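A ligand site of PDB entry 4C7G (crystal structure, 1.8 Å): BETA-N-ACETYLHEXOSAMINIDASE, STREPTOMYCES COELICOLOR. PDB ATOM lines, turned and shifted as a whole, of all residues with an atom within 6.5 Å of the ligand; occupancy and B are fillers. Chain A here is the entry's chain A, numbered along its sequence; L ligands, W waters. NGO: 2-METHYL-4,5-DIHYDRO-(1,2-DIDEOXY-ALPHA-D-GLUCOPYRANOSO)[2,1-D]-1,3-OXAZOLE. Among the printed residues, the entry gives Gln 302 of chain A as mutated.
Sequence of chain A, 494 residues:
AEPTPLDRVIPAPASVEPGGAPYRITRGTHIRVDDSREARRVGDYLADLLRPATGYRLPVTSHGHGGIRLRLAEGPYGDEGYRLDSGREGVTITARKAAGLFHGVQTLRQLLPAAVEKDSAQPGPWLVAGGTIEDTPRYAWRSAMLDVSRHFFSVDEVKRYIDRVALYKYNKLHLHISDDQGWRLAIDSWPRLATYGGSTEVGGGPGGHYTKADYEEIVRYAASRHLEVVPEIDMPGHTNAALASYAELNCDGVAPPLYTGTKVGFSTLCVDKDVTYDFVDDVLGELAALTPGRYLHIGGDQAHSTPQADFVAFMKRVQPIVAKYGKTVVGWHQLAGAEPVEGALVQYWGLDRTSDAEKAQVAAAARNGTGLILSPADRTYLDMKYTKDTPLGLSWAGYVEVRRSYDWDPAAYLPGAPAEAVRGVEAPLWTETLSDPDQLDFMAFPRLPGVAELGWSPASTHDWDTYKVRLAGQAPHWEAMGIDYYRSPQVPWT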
ATOM      1  N   ASP A 147     -15.083 -25.996   9.637  1.00  0.00           N
ATOM      2  CA  ASP A 147     -14.080 -26.939  10.173  1.00  0.00           C
ATOM      3  C   ASP A 147     -14.823 -27.816  11.174  1.00  0.00           C
ATOM      4  O   ASP A 147     -15.284 -27.344  12.241  1.00  0.00           O
ATOM      5  CB  ASP A 147     -13.071 -26.036  10.902  1.00  0.00           C
ATOM      6  CG  ASP A 147     -11.993 -26.788  11.667  1.00  0.00           C
ATOM      7  OD1 ASP A 147     -11.969 -28.047  11.738  1.00  0.00           O
ATOM      8  OD2 ASP A 147     -11.143 -26.054  12.205  1.00  0.00           O
ATOM      9  N   ARG A 150     -11.469 -29.515  14.207  1.00  0.00           N
ATOM     10  CA  ARG A 150     -11.014 -28.974  15.484  1.00  0.00           C
ATOM     11  C   ARG A 150     -12.030 -29.224  16.609  1.00  0.00           C
ATOM     12  O   ARG A 150     -11.683 -29.654  17.702  1.00  0.00           O
ATOM     13  CB  ARG A 150     -10.694 -27.479  15.312  1.00  0.00           C
ATOM     14  CG  ARG A 150      -9.233 -27.273  14.864  1.00  0.00           C
ATOM     15  CD  ARG A 150      -8.874 -28.039  13.568  1.00  0.00           C
ATOM     16  NE  ARG A 150      -7.491 -27.718  13.176  1.00  0.00           N
ATOM     17  CZ  ARG A 150      -7.125 -26.666  12.426  1.00  0.00           C
ATOM     18  NH1 ARG A 150      -8.119 -25.864  11.917  1.00  0.00           N
ATOM     19  NH2 ARG A 150      -5.786 -26.425  12.145  1.00  0.00           N
ATOM     20  N   HIS A 176     -14.224 -29.215   6.063  1.00  0.00           N
ATOM     21  CA  HIS A 176     -12.843 -29.554   6.412  1.00  0.00           C
ATOM     22  C   HIS A 176     -12.929 -30.705   7.421  1.00  0.00           C
ATOM     23  O   HIS A 176     -13.086 -30.492   8.619  1.00  0.00           O
ATOM     24  CB  HIS A 176     -12.175 -28.255   6.947  1.00  0.00           C
ATOM     25  CG  HIS A 176     -10.738 -28.415   7.284  1.00  0.00           C
ATOM     26  ND1 HIS A 176      -9.747 -28.209   6.356  1.00  0.00           N
ATOM     27  CD2 HIS A 176     -10.125 -28.749   8.454  1.00  0.00           C
ATOM     28  CE1 HIS A 176      -8.562 -28.414   6.933  1.00  0.00           C
ATOM     29  NE2 HIS A 176      -8.764 -28.743   8.209  1.00  0.00           N
ATOM     30  N   ASP A 179      -8.055 -33.153  10.166  1.00  0.00           N
ATOM     31  CA  ASP A 179      -6.953 -32.265  10.631  1.00  0.00           C
ATOM     32  C   ASP A 179      -6.108 -32.991  11.652  1.00  0.00           C
ATOM     33  O   ASP A 179      -6.151 -34.240  11.795  1.00  0.00           O
ATOM     34  CB  ASP A 179      -7.494 -30.894  11.140  1.00  0.00           C
ATOM     35  CG  ASP A 179      -6.501 -29.756  10.845  1.00  0.00           C
ATOM     36  OD1 ASP A 179      -5.473 -29.791  11.549  1.00  0.00           O
ATOM     37  OD2 ASP A 179      -6.710 -28.948   9.875  1.00  0.00           O
ATOM     38  N   ASP A 234      -7.076 -32.875   4.259  1.00  0.00           N
ATOM     39  CA  ASP A 234      -5.925 -31.933   4.109  1.00  0.00           C
ATOM     40  C   ASP A 234      -4.683 -32.855   4.029  1.00  0.00           C
ATOM     41  O   ASP A 234      -4.520 -33.813   4.829  1.00  0.00           O
ATOM     42  CB  ASP A 234      -5.857 -31.111   5.410  1.00  0.00           C
ATOM     43  CG  ASP A 234      -5.018 -29.818   5.223  1.00  0.00           C
ATOM     44  OD1 ASP A 234      -4.183 -29.844   4.303  1.00  0.00           O
ATOM     45  OD2 ASP A 234      -5.284 -28.797   5.929  1.00  0.00           O
ATOM     46  N   HIS A 238      -1.199 -31.208   8.460  1.00  0.00           N
ATOM     47  CA  HIS A 238      -2.519 -31.293   9.139  1.00  0.00           C
ATOM     48  C   HIS A 238      -3.088 -32.712   9.134  1.00  0.00           C
ATOM     49  O   HIS A 238      -4.328 -32.910   8.993  1.00  0.00           O
ATOM     50  CB  HIS A 238      -3.491 -30.238   8.521  1.00  0.00           C
ATOM     51  CG  HIS A 238      -3.179 -28.851   8.995  1.00  0.00           C
ATOM     52  ND1 HIS A 238      -3.557 -28.412  10.243  1.00  0.00           N
ATOM     53  CD2 HIS A 238      -2.425 -27.861   8.440  1.00  0.00           C
ATOM     54  CE1 HIS A 238      -3.099 -27.172  10.417  1.00  0.00           C
ATOM     55  NE2 HIS A 238      -2.416 -26.813   9.356  1.00  0.00           N
ATOM     56  N   VAL A 264      -0.021 -25.596  14.886  1.00  0.00           N
ATOM     57  CA  VAL A 264      -0.020 -26.076  13.496  1.00  0.00           C
ATOM     58  C   VAL A 264       1.392 -26.360  12.957  1.00  0.00           C
ATOM     59  O   VAL A 264       2.377 -25.817  13.488  1.00  0.00           O
ATOM     60  CB  VAL A 264      -0.671 -25.048  12.531  1.00  0.00           C
ATOM     61  CG1 VAL A 264      -2.113 -24.694  13.003  1.00  0.00           C
ATOM     62  CG2 VAL A 264       0.141 -23.748  12.513  1.00  0.00           C
ATOM     63  N   ASP A 301      -2.013 -26.693   3.015  1.00  0.00           N
ATOM     64  CA  ASP A 301      -1.612 -25.589   3.908  1.00  0.00           C
ATOM     65  C   ASP A 301      -0.693 -26.038   5.060  1.00  0.00           C
ATOM     66  O   ASP A 301      -0.824 -27.167   5.547  1.00  0.00           O
ATOM     67  CB  ASP A 301      -2.872 -24.924   4.469  1.00  0.00           C
ATOM     68  CG  ASP A 301      -3.664 -25.852   5.395  1.00  0.00           C
ATOM     69  OD1 ASP A 301      -3.978 -26.959   4.927  1.00  0.00           O
ATOM     70  OD2 ASP A 301      -3.903 -25.523   6.605  1.00  0.00           O
ATOM     71  N   GLN A 302       0.280 -25.182   5.438  1.00  0.00           N
ATOM     72  CA  GLN A 302       1.055 -25.361   6.663  1.00  0.00           C
ATOM     73  C   GLN A 302       1.737 -26.748   6.758  1.00  0.00           C
ATOM     74  O   GLN A 302       1.793 -27.365   7.826  1.00  0.00           O
ATOM     75  CB  GLN A 302       0.172 -25.096   7.892  1.00  0.00           C
ATOM     76  CG  GLN A 302      -0.170 -23.605   8.003  1.00  0.00           C
ATOM     77  CD  GLN A 302      -1.189 -23.293   9.082  1.00  0.00           C
ATOM     78  OE1 GLN A 302      -1.956 -24.176   9.577  1.00  0.00           O
ATOM     79  NE2 GLN A 302      -1.140 -22.064   9.539  1.00  0.00           N
ATOM     80  N   TRP A 332      -5.191 -25.305  -1.025  1.00  0.00           N
ATOM     81  CA  TRP A 332      -4.795 -23.988  -0.489  1.00  0.00           C
ATOM     82  C   TRP A 332      -3.620 -23.472  -1.341  1.00  0.00           C
ATOM     83  O   TRP A 332      -2.989 -24.296  -2.065  1.00  0.00           O
ATOM     84  CB  TRP A 332      -4.398 -24.040   0.972  1.00  0.00           C
ATOM     85  CG  TRP A 332      -5.511 -24.539   1.834  1.00  0.00           C
ATOM     86  CD1 TRP A 332      -5.629 -25.799   2.363  1.00  0.00           C
ATOM     87  CD2 TRP A 332      -6.674 -23.807   2.254  1.00  0.00           C
ATOM     88  NE1 TRP A 332      -6.787 -25.900   3.142  1.00  0.00           N
ATOM     89  CE2 TRP A 332      -7.451 -24.696   3.068  1.00  0.00           C
ATOM     90  CE3 TRP A 332      -7.161 -22.506   1.984  1.00  0.00           C
ATOM     91  CZ2 TRP A 332      -8.685 -24.330   3.616  1.00  0.00           C
ATOM     92  CZ3 TRP A 332      -8.350 -22.098   2.630  1.00  0.00           C
ATOM     93  CH2 TRP A 332      -9.127 -23.024   3.420  1.00  0.00           C
ATOM     94  N   GLN A 334      -0.633 -22.649  -1.269  1.00  0.00           N
ATOM     95  CA  GLN A 334       0.684 -23.332  -1.279  1.00  0.00           C
ATOM     96  C   GLN A 334       0.857 -24.224  -2.478  1.00  0.00           C
ATOM     97  O   GLN A 334       2.000 -24.467  -2.938  1.00  0.00           O
ATOM     98  CB  GLN A 334       0.963 -24.105   0.021  1.00  0.00           C
ATOM     99  CG  GLN A 334       1.327 -23.146   1.151  1.00  0.00           C
ATOM    100  CD  GLN A 334       0.146 -22.280   1.615  1.00  0.00           C
ATOM    101  OE1 GLN A 334      -1.022 -22.736   1.675  1.00  0.00           O
ATOM    102  NE2 GLN A 334       0.453 -21.010   1.980  1.00  0.00           N
ATOM    103  N   TRP A 349      -5.452 -17.769   0.866  1.00  0.00           N
ATOM    104  CA  TRP A 349      -5.821 -17.436   2.224  1.00  0.00           C
ATOM    105  C   TRP A 349      -4.831 -16.471   2.831  1.00  0.00           C
ATOM    106  O   TRP A 349      -4.781 -16.293   4.054  1.00  0.00           O
ATOM    107  CB  TRP A 349      -5.942 -18.696   3.094  1.00  0.00           C
ATOM    108  CG  TRP A 349      -4.632 -19.544   3.170  1.00  0.00           C
ATOM    109  CD1 TRP A 349      -4.167 -20.446   2.220  1.00  0.00           C
ATOM    110  CD2 TRP A 349      -3.758 -19.634   4.273  1.00  0.00           C
ATOM    111  NE1 TRP A 349      -3.005 -21.061   2.722  1.00  0.00           N
ATOM    112  CE2 TRP A 349      -2.752 -20.586   3.960  1.00  0.00           C
ATOM    113  CE3 TRP A 349      -3.746 -19.016   5.553  1.00  0.00           C
ATOM    114  CZ2 TRP A 349      -1.704 -20.904   4.859  1.00  0.00           C
ATOM    115  CZ3 TRP A 349      -2.699 -19.309   6.426  1.00  0.00           C
ATOM    116  CH2 TRP A 349      -1.680 -20.246   6.099  1.00  0.00           C
ATOM    117  N   ALA A 377      -7.227 -14.149   4.771  1.00  0.00           N
ATOM    118  CA  ALA A 377      -7.436 -14.365   6.183  1.00  0.00           C
ATOM    119  C   ALA A 377      -7.775 -13.086   6.934  1.00  0.00           C
ATOM    120  O   ALA A 377      -8.316 -13.131   8.011  1.00  0.00           O
ATOM    121  CB  ALA A 377      -6.191 -15.025   6.839  1.00  0.00           C
ATOM    122  N   TYR A 381     -12.189 -14.709   6.837  1.00  0.00           N
ATOM    123  CA  TYR A 381     -12.072 -15.745   7.914  1.00  0.00           C
ATOM    124  C   TYR A 381     -13.023 -15.323   9.021  1.00  0.00           C
ATOM    125  O   TYR A 381     -12.783 -14.337   9.789  1.00  0.00           O
ATOM    126  CB  TYR A 381     -10.644 -15.875   8.478  1.00  0.00           C
ATOM    127  CG  TYR A 381      -9.753 -16.867   7.763  1.00  0.00           C
ATOM    128  CD1 TYR A 381      -9.802 -17.020   6.384  1.00  0.00           C
ATOM    129  CD2 TYR A 381      -8.837 -17.641   8.485  1.00  0.00           C
ATOM    130  CE1 TYR A 381      -8.961 -17.929   5.735  1.00  0.00           C
ATOM    131  CE2 TYR A 381      -8.002 -18.545   7.841  1.00  0.00           C
ATOM    132  CZ  TYR A 381      -8.068 -18.663   6.483  1.00  0.00           C
ATOM    133  OH  TYR A 381      -7.288 -19.627   5.822  1.00  0.00           O
ATOM    134  N   ASP A 383     -13.512 -16.921  11.739  1.00  0.00           N
ATOM    135  CA  ASP A 383     -12.988 -17.171  13.113  1.00  0.00           C
ATOM    136  C   ASP A 383     -12.090 -16.044  13.600  1.00  0.00           C
ATOM    137  O   ASP A 383     -11.669 -16.111  14.762  1.00  0.00           O
ATOM    138  CB  ASP A 383     -12.133 -18.470  13.187  1.00  0.00           C
ATOM    139  CG  ASP A 383     -10.965 -18.448  12.210  1.00  0.00           C
ATOM    140  OD1 ASP A 383     -11.191 -18.090  11.020  1.00  0.00           O
ATOM    141  OD2 ASP A 383      -9.853 -18.845  12.616  1.00  0.00           O
ATOM    142  N   MET A 384     -11.840 -15.056  12.734  1.00  0.00           N
ATOM    143  CA  MET A 384     -10.993 -13.905  13.091  1.00  0.00           C
ATOM    144  C   MET A 384     -11.786 -12.934  13.996  1.00  0.00           C
ATOM    145  O   MET A 384     -12.922 -12.582  13.658  1.00  0.00           O
ATOM    146  CB  MET A 384     -10.365 -13.202  11.887  1.00  0.00           C
ATOM    147  CG  MET A 384      -8.952 -12.651  12.183  1.00  0.00           C
ATOM    148  SD  MET A 384      -7.760 -14.028  12.495  1.00  0.00           S
ATOM    149  CE  MET A 384      -7.987 -15.055  11.037  1.00  0.00           C
ATOM    150  N   LEU A 394      -9.670 -16.012  16.704  1.00  0.00           N
ATOM    151  CA  LEU A 394      -8.231 -15.818  16.732  1.00  0.00           C
ATOM    152  C   LEU A 394      -7.895 -14.393  16.246  1.00  0.00           C
ATOM    153  O   LEU A 394      -8.774 -13.694  15.702  1.00  0.00           O
ATOM    154  CB  LEU A 394      -7.549 -16.834  15.796  1.00  0.00           C
ATOM    155  CG  LEU A 394      -7.717 -18.302  16.242  1.00  0.00           C
ATOM    156  CD1 LEU A 394      -7.065 -19.224  15.178  1.00  0.00           C
ATOM    157  CD2 LEU A 394      -7.236 -18.583  17.684  1.00  0.00           C
ATOM    158  N   TRP A 396      -4.543 -13.936  14.680  1.00  0.00           N
ATOM    159  CA  TRP A 396      -3.266 -14.076  13.979  1.00  0.00           C
ATOM    160  C   TRP A 396      -3.206 -13.246  12.717  1.00  0.00           C
ATOM    161  O   TRP A 396      -2.104 -12.816  12.305  1.00  0.00           O
ATOM    162  CB  TRP A 396      -2.929 -15.549  13.653  1.00  0.00           C
ATOM    163  CG  TRP A 396      -3.803 -16.203  12.570  1.00  0.00           C
ATOM    164  CD1 TRP A 396      -4.908 -17.007  12.769  1.00  0.00           C
ATOM    165  CD2 TRP A 396      -3.554 -16.185  11.184  1.00  0.00           C
ATOM    166  NE1 TRP A 396      -5.384 -17.437  11.553  1.00  0.00           N
ATOM    167  CE2 TRP A 396      -4.582 -16.942  10.564  1.00  0.00           C
ATOM    168  CE3 TRP A 396      -2.583 -15.565  10.365  1.00  0.00           C
ATOM    169  CZ2 TRP A 396      -4.642 -17.111   9.185  1.00  0.00           C
ATOM    170  CZ3 TRP A 396      -2.650 -15.718   9.019  1.00  0.00           C
ATOM    171  CH2 TRP A 396      -3.656 -16.501   8.414  1.00  0.00           C
ATOM    172  N   TRP A 430     -13.132 -21.551  10.875  1.00  0.00           N
ATOM    173  CA  TRP A 430     -12.258 -22.514  11.563  1.00  0.00           C
ATOM    174  C   TRP A 430     -12.703 -22.627  13.001  1.00  0.00           C
ATOM    175  O   TRP A 430     -13.303 -21.702  13.558  1.00  0.00           O
ATOM    176  CB  TRP A 430     -10.803 -22.027  11.533  1.00  0.00           C
ATOM    177  CG  TRP A 430     -10.312 -21.897  10.160  1.00  0.00           C
ATOM    178  CD1 TRP A 430     -10.236 -20.753   9.412  1.00  0.00           C
ATOM    179  CD2 TRP A 430      -9.783 -22.942   9.350  1.00  0.00           C
ATOM    180  NE1 TRP A 430      -9.728 -21.050   8.149  1.00  0.00           N
ATOM    181  CE2 TRP A 430      -9.449 -22.388   8.099  1.00  0.00           C
ATOM    182  CE3 TRP A 430      -9.649 -24.338   9.540  1.00  0.00           C
ATOM    183  CZ2 TRP A 430      -8.876 -23.169   7.067  1.00  0.00           C
ATOM    184  CZ3 TRP A 430      -9.092 -25.085   8.551  1.00  0.00           C
ATOM    185  CH2 TRP A 430      -8.748 -24.525   7.309  1.00  0.00           C
ATOM    186  N   THR A 431     -12.478 -23.784  13.629  1.00  0.00           N
ATOM    187  CA  THR A 431     -13.127 -24.035  14.922  1.00  0.00           C
ATOM    188  C   THR A 431     -12.207 -24.388  16.119  1.00  0.00           C
ATOM    189  O   THR A 431     -12.647 -25.062  17.110  1.00  0.00           O
ATOM    190  CB  THR A 431     -14.293 -25.051  14.795  1.00  0.00           C
ATOM    191  OG1 THR A 431     -13.785 -26.277  14.260  1.00  0.00           O
ATOM    192  CG2 THR A 431     -15.384 -24.520  13.852  1.00  0.00           C
ATOM    193  N   GLU A 432     -10.924 -23.939  16.068  1.00  0.00           N
ATOM    194  CA  GLU A 432     -10.075 -24.072  17.273  1.00  0.00           C
ATOM    195  C   GLU A 432     -10.818 -23.588  18.544  1.00  0.00           C
ATOM    196  O   GLU A 432     -10.668 -24.161  19.639  1.00  0.00           O
ATOM    197  CB  GLU A 432      -8.793 -23.209  17.123  1.00  0.00           C
ATOM    198  CG  GLU A 432      -7.675 -23.797  16.261  1.00  0.00           C
ATOM    199  CD  GLU A 432      -7.785 -23.396  14.804  1.00  0.00           C
ATOM    200  OE1 GLU A 432      -8.918 -23.070  14.302  1.00  0.00           O
ATOM    201  OE2 GLU A 432      -6.731 -23.382  14.140  1.00  0.00           O
HETATM  202  C1  NGO L   1      -5.027 -20.944   8.680  1.00  0.00           C
HETATM  203  C2  NGO L   1      -4.473 -22.376   8.894  1.00  0.00           C
HETATM  204  C3  NGO L   1      -5.397 -23.261   9.736  1.00  0.00           C
HETATM  205  C4  NGO L   1      -5.949 -22.520  10.967  1.00  0.00           C
HETATM  206  C5  NGO L   1      -6.676 -21.233  10.484  1.00  0.00           C
HETATM  207  C6  NGO L   1      -7.228 -20.467  11.712  1.00  0.00           C
HETATM  208  C7  NGO L   1      -5.201 -22.151   6.734  1.00  0.00           C
HETATM  209  C8  NGO L   1      -5.482 -22.436   5.320  1.00  0.00           C
HETATM  210  N2  NGO L   1      -4.355 -22.828   7.502  1.00  0.00           N
HETATM  211  O1  NGO L   1      -5.779 -21.060   7.491  1.00  0.00           O
HETATM  212  O3  NGO L   1      -4.632 -24.367  10.218  1.00  0.00           O
HETATM  213  O4  NGO L   1      -6.928 -23.341  11.637  1.00  0.00           O
HETATM  214  O5  NGO L   1      -5.745 -20.378   9.756  1.00  0.00           O
HETATM  215  O6  NGO L   1      -7.635 -19.136  11.272  1.00  0.00           O
HETATM  216  O   HOH W   1      -5.802 -26.601   8.595  1.00  0.00           O
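The side-chain carboxylate (OE2) of Glu 432 is in salt-bridge range of the guanidinium group (NH1) of Arg 150 (3.6 Å). O of Asp 383 is in hydrogen-bond range of N of Leu 394 (2.8 Å). The side-chain amide oxygen (OE1) of Gln 302 sits at hydrogen-bond distance from a ring nitrogen (NE2) of His 238 (2.7 Å). NE of Arg 150 is in salt-bridge range of OD1 of Asp 179, at 3.3 Å. The side-chain carboxylate of Asp 301 sits close to the indole nitrogen of Trp 332 (3.5 Å). The side-chain carboxylate (OD1) of Asp 301 sits close to the side-chain carboxylate (OD2) of Asp 234 (2.5 Å). A ring nitrogen (ND1) of His 238 is in hydrogen-bond range of the side-chain carboxylate (OD1) of Asp 179. The backbone NH (N) of Ala 377 is in hydrogen-bond range of the backbone carbonyl oxygen (O) of Trp 349, at 3.3 Å.
Merely in contact with the ligand: Val 264, Trp 332, Trp 349, Leu 394 and Trp 430. Hydrophobic or aromatic side chains within 4 Å of the ligand: His 238, Val 264, Trp 332, Trp 349, Tyr 381, Leu 394, Trp 396 and Trp 430. The nearest printed residue that does not touch the ligand is Met 384 (4.1 Å).
OE2 of Glu 432 is in hydrogen-bond range of O4 of the ligand (2.5 Å). An oxygen (O6) of the ligand lies within hydrogen-bond range of the side-chain carboxylate of Asp 383, at 2.6 Å. An oxygen (O1) of the ligand sits at hydrogen-bond distance from the side-chain hydroxyl (OH) of Tyr 381 (2.7 Å). The side-chain amide oxygen (OE1) of Gln 302 sits at hydrogen-bond distance from an oxygen (O3) of the ligand (2.8 Å). An oxygen (O4) of the ligand sits at hydrogen-bond distance from the guanidinium group of Arg 150, 2.8 Å away. NE1 of Trp 396 sits at hydrogen-bond distance from O6 of the ligand, 2.8 Å away. OD2 of Asp 301 lies within salt-bridge range of N2 of the ligand (2.9 Å). An oxygen (O3) of the ligand lies close to a ring nitrogen (NE2) of His 238, 3.4 Å away.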
